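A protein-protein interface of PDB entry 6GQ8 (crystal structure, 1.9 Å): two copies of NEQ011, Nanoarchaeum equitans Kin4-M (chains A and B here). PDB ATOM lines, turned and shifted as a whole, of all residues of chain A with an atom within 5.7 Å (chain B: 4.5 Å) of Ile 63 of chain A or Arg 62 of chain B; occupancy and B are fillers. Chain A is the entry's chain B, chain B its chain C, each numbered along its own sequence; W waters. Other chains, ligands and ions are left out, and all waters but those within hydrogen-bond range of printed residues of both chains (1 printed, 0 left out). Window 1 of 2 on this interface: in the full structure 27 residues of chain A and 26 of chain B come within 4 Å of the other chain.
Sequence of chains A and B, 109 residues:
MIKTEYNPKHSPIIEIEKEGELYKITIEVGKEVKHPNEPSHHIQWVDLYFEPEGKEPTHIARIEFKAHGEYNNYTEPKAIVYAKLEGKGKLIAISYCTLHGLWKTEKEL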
ATOM      1  N   ILE A  27      12.319  18.676  16.743  1.00  0.00           N
ATOM      2  CA  ILE A  27      11.193  17.825  17.109  1.00  0.00           C
ATOM      3  C   ILE A  27       9.956  18.705  17.221  1.00  0.00           C
ATOM      4  O   ILE A  27       9.982  19.730  17.910  1.00  0.00           O
ATOM      5  CB  ILE A  27      11.443  17.064  18.426  1.00  0.00           C
ATOM      6  CG1 ILE A  27      12.797  16.352  18.389  1.00  0.00           C
ATOM      7  CG2 ILE A  27      10.333  16.055  18.673  1.00  0.00           C
ATOM      8  CD1 ILE A  27      13.409  16.135  19.753  1.00  0.00           C
ATOM      9  N   GLN A  44       2.857  17.728  26.815  1.00  0.00           N
ATOM     10  CA  GLN A  44       3.592  18.120  28.011  1.00  0.00           C
ATOM     11  C   GLN A  44       5.105  18.060  27.827  1.00  0.00           C
ATOM     12  O   GLN A  44       5.817  18.952  28.302  1.00  0.00           O
ATOM     13  CB  GLN A  44       3.169  17.241  29.191  1.00  0.00           C
ATOM     14  CG  GLN A  44       3.516  17.819  30.552  1.00  0.00           C
ATOM     15  CD  GLN A  44       2.882  17.038  31.693  1.00  0.00           C
ATOM     16  OE1 GLN A  44       3.378  15.984  32.092  1.00  0.00           O
ATOM     17  NE2 GLN A  44       1.775  17.554  32.219  1.00  0.00           N
ATOM     18  N   TRP A  45       5.617  17.033  27.155  1.00  0.00           N
ATOM     19  CA  TRP A  45       7.062  16.871  27.036  1.00  0.00           C
ATOM     20  C   TRP A  45       7.380  15.955  25.863  1.00  0.00           C
ATOM     21  O   TRP A  45       6.503  15.303  25.294  1.00  0.00           O
ATOM     22  CB  TRP A  45       7.673  16.331  28.338  1.00  0.00           C
ATOM     23  CG  TRP A  45       7.046  15.062  28.877  1.00  0.00           C
ATOM     24  CD1 TRP A  45       6.090  14.971  29.851  1.00  0.00           C
ATOM     25  CD2 TRP A  45       7.367  13.712  28.506  1.00  0.00           C
ATOM     26  NE1 TRP A  45       5.781  13.653  30.090  1.00  0.00           N
ATOM     27  CE2 TRP A  45       6.555  12.861  29.283  1.00  0.00           C
ATOM     28  CE3 TRP A  45       8.254  13.141  27.586  1.00  0.00           C
ATOM     29  CZ2 TRP A  45       6.596  11.472  29.160  1.00  0.00           C
ATOM     30  CZ3 TRP A  45       8.297  11.759  27.471  1.00  0.00           C
ATOM     31  CH2 TRP A  45       7.478  10.943  28.256  1.00  0.00           C
ATOM     32  N   VAL A  46       8.662  15.927  25.506  1.00  0.00           N
ATOM     33  CA  VAL A  46       9.193  14.988  24.526  1.00  0.00           C
ATOM     34  C   VAL A  46      10.576  14.548  24.998  1.00  0.00           C
ATOM     35  O   VAL A  46      11.372  15.374  25.456  1.00  0.00           O
ATOM     36  CB  VAL A  46       9.251  15.595  23.107  1.00  0.00           C
ATOM     37  CG1 VAL A  46      10.006  16.919  23.104  1.00  0.00           C
ATOM     38  CG2 VAL A  46       9.883  14.614  22.127  1.00  0.00           C
ATOM     39  N   ASP A  47      10.839  13.246  24.933  1.00  0.00           N
ATOM     40  CA  ASP A  47      12.160  12.685  25.198  1.00  0.00           C
ATOM     41  C   ASP A  47      12.808  12.286  23.880  1.00  0.00           C
ATOM     42  O   ASP A  47      12.150  11.718  23.005  1.00  0.00           O
ATOM     43  CB  ASP A  47      12.076  11.463  26.121  1.00  0.00           C
ATOM     44  CG  ASP A  47      12.095  11.825  27.601  1.00  0.00           C
ATOM     45  OD1 ASP A  47      12.733  12.828  27.977  1.00  0.00           O
ATOM     46  OD2 ASP A  47      11.475  11.093  28.397  1.00  0.00           O
ATOM     47  N   LEU A  48      14.099  12.584  23.739  1.00  0.00           N
ATOM     48  CA  LEU A  48      14.849  12.252  22.533  1.00  0.00           C
ATOM     49  C   LEU A  48      15.957  11.276  22.889  1.00  0.00           C
ATOM     50  O   LEU A  48      16.807  11.577  23.733  1.00  0.00           O
ATOM     51  CB  LEU A  48      15.437  13.504  21.880  1.00  0.00           C
ATOM     52  CG  LEU A  48      16.302  13.224  20.650  1.00  0.00           C
ATOM     53  CD1 LEU A  48      15.444  12.701  19.510  1.00  0.00           C
ATOM     54  CD2 LEU A  48      17.066  14.467  20.224  1.00  0.00           C
ATOM     55  N   ALA A  61      18.048  14.196  25.080  1.00  0.00           N
ATOM     56  CA  ALA A  61      17.453  15.416  25.602  1.00  0.00           C
ATOM     57  C   ALA A  61      16.096  15.108  26.211  1.00  0.00           C
ATOM     58  O   ALA A  61      15.428  14.146  25.827  1.00  0.00           O
ATOM     59  CB  ALA A  61      17.301  16.489  24.518  1.00  0.00           C
ATOM     60  N   ARG A  62      15.714  15.933  27.182  1.00  0.00           N
ATOM     61  CA  ARG A  62      14.375  15.939  27.760  1.00  0.00           C
ATOM     62  C   ARG A  62      13.886  17.376  27.749  1.00  0.00           C
ATOM     63  O   ARG A  62      14.549  18.258  28.304  1.00  0.00           O
ATOM     64  CB  ARG A  62      14.385  15.373  29.184  1.00  0.00           C
ATOM     65  CG  ARG A  62      13.076  15.522  29.949  1.00  0.00           C
ATOM     66  CD  ARG A  62      13.061  14.596  31.160  1.00  0.00           C
ATOM     67  NE  ARG A  62      12.752  13.226  30.766  1.00  0.00           N
ATOM     68  CZ  ARG A  62      12.815  12.174  31.572  1.00  0.00           C
ATOM     69  NH1 ARG A  62      13.193  12.321  32.838  1.00  0.00           N
ATOM     70  NH2 ARG A  62      12.503  10.971  31.107  1.00  0.00           N
ATOM     71  N   ILE A  63      12.755  17.619  27.090  1.00  0.00           N
ATOM     72  CA  ILE A  63      12.203  18.961  26.936  1.00  0.00           C
ATOM     73  C   ILE A  63      10.784  18.958  27.480  1.00  0.00           C
ATOM     74  O   ILE A  63       9.933  18.202  26.998  1.00  0.00           O
ATOM     75  CB  ILE A  63      12.221  19.427  25.474  1.00  0.00           C
ATOM     76  CG1 ILE A  63      13.640  19.340  24.908  1.00  0.00           C
ATOM     77  CG2 ILE A  63      11.676  20.842  25.366  1.00  0.00           C
ATOM     78  CD1 ILE A  63      13.824  18.233  23.909  1.00  0.00           C
ATOM     79  N   GLU A  64      10.527  19.810  28.467  1.00  0.00           N
ATOM     80  CA  GLU A  64       9.200  19.980  29.044  1.00  0.00           C
ATOM     81  C   GLU A  64       8.614  21.291  28.539  1.00  0.00           C
ATOM     82  O   GLU A  64       9.235  22.348  28.690  1.00  0.00           O
ATOM     83  CB  GLU A  64       9.268  19.976  30.572  1.00  0.00           C
ATOM     84  CG  GLU A  64       9.923  18.736  31.157  1.00  0.00           C
ATOM     85  CD  GLU A  64       8.919  17.766  31.748  1.00  0.00           C
ATOM     86  OE1 GLU A  64       7.702  18.031  31.646  1.00  0.00           O
ATOM     87  OE2 GLU A  64       9.350  16.736  32.311  1.00  0.00           O
ATOM     88  N   PHE A  65       7.427  21.218  27.939  1.00  0.00           N
ATOM     89  CA  PHE A  65       6.688  22.400  27.506  1.00  0.00           C
ATOM     90  C   PHE A  65       5.726  22.795  28.624  1.00  0.00           C
ATOM     91  O   PHE A  65       4.722  22.114  28.856  1.00  0.00           O
ATOM     92  CB  PHE A  65       5.949  22.118  26.202  1.00  0.00           C
ATOM     93  CG  PHE A  65       6.794  21.438  25.158  1.00  0.00           C
ATOM     94  CD1 PHE A  65       7.837  22.111  24.544  1.00  0.00           C
ATOM     95  CD2 PHE A  65       6.540  20.129  24.786  1.00  0.00           C
ATOM     96  CE1 PHE A  65       8.608  21.495  23.583  1.00  0.00           C
ATOM     97  CE2 PHE A  65       7.311  19.504  23.826  1.00  0.00           C
ATOM     98  CZ  PHE A  65       8.346  20.191  23.222  1.00  0.00           C
ATOM     99  N   LYS A  66       6.024  23.901  29.308  1.00  0.00           N
ATOM    100  CA  LYS A  66       5.479  24.148  30.639  1.00  0.00           C
ATOM    101  C   LYS A  66       4.248  25.046  30.678  1.00  0.00           C
ATOM    102  O   LYS A  66       3.449  24.920  31.612  1.00  0.00           O
ATOM    103  CB  LYS A  66       6.562  24.757  31.537  1.00  0.00           C
ATOM    104  CG  LYS A  66       7.689  23.791  31.894  1.00  0.00           C
ATOM    105  CD  LYS A  66       7.156  22.607  32.673  1.00  0.00           C
ATOM    106  CE  LYS A  66       8.184  22.056  33.641  1.00  0.00           C
ATOM    107  NZ  LYS A  66       7.589  20.948  34.428  1.00  0.00           N
ATOM    108  N   ALA A  79      10.827  21.877  19.619  1.00  0.00           N
ATOM    109  CA  ALA A  79      12.123  22.141  20.219  1.00  0.00           C
ATOM    110  C   ALA A  79      13.219  21.742  19.244  1.00  0.00           C
ATOM    111  O   ALA A  79      13.051  20.825  18.437  1.00  0.00           O
ATOM    112  CB  ALA A  79      12.293  21.385  21.543  1.00  0.00           C
ATOM    113  N   VAL A  81      17.318  20.751  19.452  1.00  0.00           N
ATOM    114  CA  VAL A  81      18.436  20.415  20.318  1.00  0.00           C
ATOM    115  C   VAL A  81      19.638  20.083  19.441  1.00  0.00           C
ATOM    116  O   VAL A  81      19.525  19.946  18.224  1.00  0.00           O
ATOM    117  CB  VAL A  81      18.108  19.258  21.280  1.00  0.00           C
ATOM    118  CG1 VAL A  81      16.987  19.663  22.231  1.00  0.00           C
ATOM    119  CG2 VAL A  81      17.718  18.020  20.505  1.00  0.00           C
ATOM    120  N   VAL B  46      18.585  23.878  31.473  1.00  0.00           N
ATOM    121  CA  VAL B  46      18.227  25.291  31.454  1.00  0.00           C
ATOM    122  C   VAL B  46      16.719  25.405  31.632  1.00  0.00           C
ATOM    123  O   VAL B  46      15.951  24.672  31.001  1.00  0.00           O
ATOM    124  CB  VAL B  46      18.693  25.995  30.161  1.00  0.00           C
ATOM    125  CG1 VAL B  46      18.150  25.290  28.924  1.00  0.00           C
ATOM    126  CG2 VAL B  46      18.284  27.461  30.176  1.00  0.00           C
ATOM    127  N   ASP B  47      16.299  26.303  32.520  1.00  0.00           N
ATOM    128  CA  ASP B  47      14.891  26.626  32.712  1.00  0.00           C
ATOM    129  C   ASP B  47      14.623  27.999  32.111  1.00  0.00           C
ATOM    130  O   ASP B  47      15.412  28.929  32.302  1.00  0.00           O
ATOM    131  CB  ASP B  47      14.506  26.630  34.199  1.00  0.00           C
ATOM    132  CG  ASP B  47      14.124  25.252  34.719  1.00  0.00           C
ATOM    133  OD1 ASP B  47      13.587  24.440  33.943  1.00  0.00           O
ATOM    134  OD2 ASP B  47      14.350  24.984  35.916  1.00  0.00           O
ATOM    135  N   HIS B  59       6.650  29.630  34.077  1.00  0.00           N
ATOM    136  CA  HIS B  59       7.601  28.662  33.545  1.00  0.00           C
ATOM    137  C   HIS B  59       7.220  28.303  32.114  1.00  0.00           C
ATOM    138  O   HIS B  59       6.101  27.843  31.862  1.00  0.00           O
ATOM    139  CB  HIS B  59       7.627  27.418  34.427  1.00  0.00           C
ATOM    140  CG  HIS B  59       8.893  26.627  34.319  1.00  0.00           C
ATOM    141  ND1 HIS B  59       9.184  25.572  35.157  1.00  0.00           N
ATOM    142  CD2 HIS B  59       9.945  26.738  33.473  1.00  0.00           C
ATOM    143  CE1 HIS B  59      10.361  25.066  34.831  1.00  0.00           C
ATOM    144  NE2 HIS B  59      10.844  25.756  33.813  1.00  0.00           N
ATOM    145  N   ALA B  61       9.692  26.681  29.594  1.00  0.00           N
ATOM    146  CA  ALA B  61      10.309  25.451  29.126  1.00  0.00           C
ATOM    147  C   ALA B  61      11.337  24.978  30.139  1.00  0.00           C
ATOM    148  O   ALA B  61      11.909  25.773  30.888  1.00  0.00           O
ATOM    149  CB  ALA B  61      10.971  25.628  27.755  1.00  0.00           C
ATOM    150  N   ARG B  62      11.546  23.665  30.158  1.00  0.00           N
ATOM    151  CA  ARG B  62      12.618  23.028  30.912  1.00  0.00           C
ATOM    152  C   ARG B  62      13.338  22.087  29.958  1.00  0.00           C
ATOM    153  O   ARG B  62      12.709  21.204  29.368  1.00  0.00           O
ATOM    154  CB  ARG B  62      12.062  22.278  32.127  1.00  0.00           C
ATOM    155  CG  ARG B  62      13.066  21.409  32.863  1.00  0.00           C
ATOM    156  CD  ARG B  62      12.551  21.027  34.247  1.00  0.00           C
ATOM    157  NE  ARG B  62      12.740  22.097  35.225  1.00  0.00           N
ATOM    158  CZ  ARG B  62      12.254  22.081  36.465  1.00  0.00           C
ATOM    159  NH1 ARG B  62      11.531  21.052  36.889  1.00  0.00           N
ATOM    160  NH2 ARG B  62      12.490  23.097  37.285  1.00  0.00           N
ATOM    161  N   ILE B  63      14.641  22.291  29.785  1.00  0.00           N
ATOM    162  CA  ILE B  63      15.432  21.525  28.827  1.00  0.00           C
ATOM    163  C   ILE B  63      16.567  20.851  29.578  1.00  0.00           C
ATOM    164  O   ILE B  63      17.377  21.526  30.222  1.00  0.00           O
ATOM    165  CB  ILE B  63      15.990  22.409  27.700  1.00  0.00           C
ATOM    166  CG1 ILE B  63      14.863  23.188  27.018  1.00  0.00           C
ATOM    167  CG2 ILE B  63      16.731  21.556  26.682  1.00  0.00           C
ATOM    168  CD1 ILE B  63      14.892  24.666  27.332  1.00  0.00           C
ATOM    169  N   GLU B  64      16.625  19.527  29.498  1.00  0.00           N
ATOM    170  CA  GLU B  64      17.707  18.754  30.090  1.00  0.00           C
ATOM    171  C   GLU B  64      18.633  18.262  28.986  1.00  0.00           C
ATOM    172  O   GLU B  64      18.180  17.623  28.031  1.00  0.00           O
ATOM    173  CB  GLU B  64      17.162  17.570  30.894  1.00  0.00           C
ATOM    174  CG  GLU B  64      16.165  17.969  31.974  1.00  0.00           C
ATOM    175  CD  GLU B  64      16.750  17.932  33.373  1.00  0.00           C
ATOM    176  OE1 GLU B  64      17.958  17.647  33.516  1.00  0.00           O
ATOM    177  OE2 GLU B  64      15.999  18.196  34.335  1.00  0.00           O
HETATM  178  O   HOH W   1       3.770  27.355  33.589  1.00  0.00           O
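The backbone carbonyl oxygen (O) of Arg 62 of chain A lies within hydrogen-bond range of the backbone NH (N) of Glu 64 of chain B (2.7 Å).
The backbone carbonyl oxygen (O) of Arg 62 of chain B lies within hydrogen-bond range of the backbone NH (N) of Glu 64 of chain A, 2.7 Å away.
The backbone NH (N) of Val 46 of chain A is in hydrogen-bond range of the backbone carbonyl oxygen (O) of Ile 63 of chain A, at 3.0 Å.
The guanidinium group of Arg 62 of chain A lies within salt-bridge range of the side-chain carboxylate of Asp 47 of chain A (2.8 Å).
The backbone NH of Leu 48 of chain A lies within hydrogen-bond range of the backbone carbonyl oxygen of Ala 61 of chain A.
The side-chain carboxylate (OD1) of Asp 47 of chain B lies within hydrogen-bond range of a ring nitrogen (NE2) of His 59 of chain B, at 3.0 Å.
The side-chain carboxylate of Asp 47 of chain B lies within salt-bridge range of the guanidinium group of Arg 62 of chain B, 2.8 Å away.
The backbone carbonyl oxygen (O) of Ala 61 of chain B sits at hydrogen-bond distance from a ring nitrogen (NE2) of His 59 of chain B.
Among the printed residues, merely in contact across the chains: Ala 61 of chain A with Glu 64 of chain B, Arg 62 of chain A with Arg 62 of chain B, Arg 62 of chain A with Ile 63 of chain B, Ile 63 of chain A with Arg 62 of chain B, Glu 64 of chain A with Ala 61 of chain B and Lys 66 of chain A with His 59 of chain B.
Of chain B, only Arg 62 (3.3 Å) comes within 4 Å of Ile 63 of chain A.
Arg 62 of chain B touches three residues of chain A.
Of the printed residues of chain A, His 59 of chain B touches Lys 66 (3.1 Å).
Printed residues of chain B within 4 Å of Ala 61 of chain A: Glu 64 (3.4 Å).
Val 81 of chain A touches none of the printed residues of chain B.
The nearest printed residue of chain A that does not touch Glu 64 of chain B is Ile 63 of chain A (4.9 Å).
Of the 14 printed residues of chain A, 5 touch a printed residue of chain B.
Hydrophobic or aromatic side chains of chain B within 4 Å of the printed part of chain A: His 59 and Ala 61.
Among the printed residues, no Asp or Glu carboxylate lies within 4 Å of a Lys or Arg side-chain nitrogen of the other chain.
Ala 61 of chain A touches Glu 64 of chain B, and with the chains exchanged Glu 64 of chain A touches Ala 61 of chain B.
Arg 62 of chain A touches its own counterpart, Arg 62 of chain B.
Arg 62 of chain A touches Ile 63 of chain B, and with the chains exchanged Ile 63 of chain A touches Arg 62 of chain B.
Arg 62 of chain A touches Glu 64 of chain B, and with the chains exchanged Glu 64 of chain A touches Arg 62 of chain B.
6 positions are printed for both chains.
Of the 8 pairs that touch across the chains among the printed residues, 7 have their exchanged pair printed and touching as well.
Water W1 lies within hydrogen-bond range of O of His 59 of chain B (2.9 Å) and O of Lys 66 of chain A (3.2 Å).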
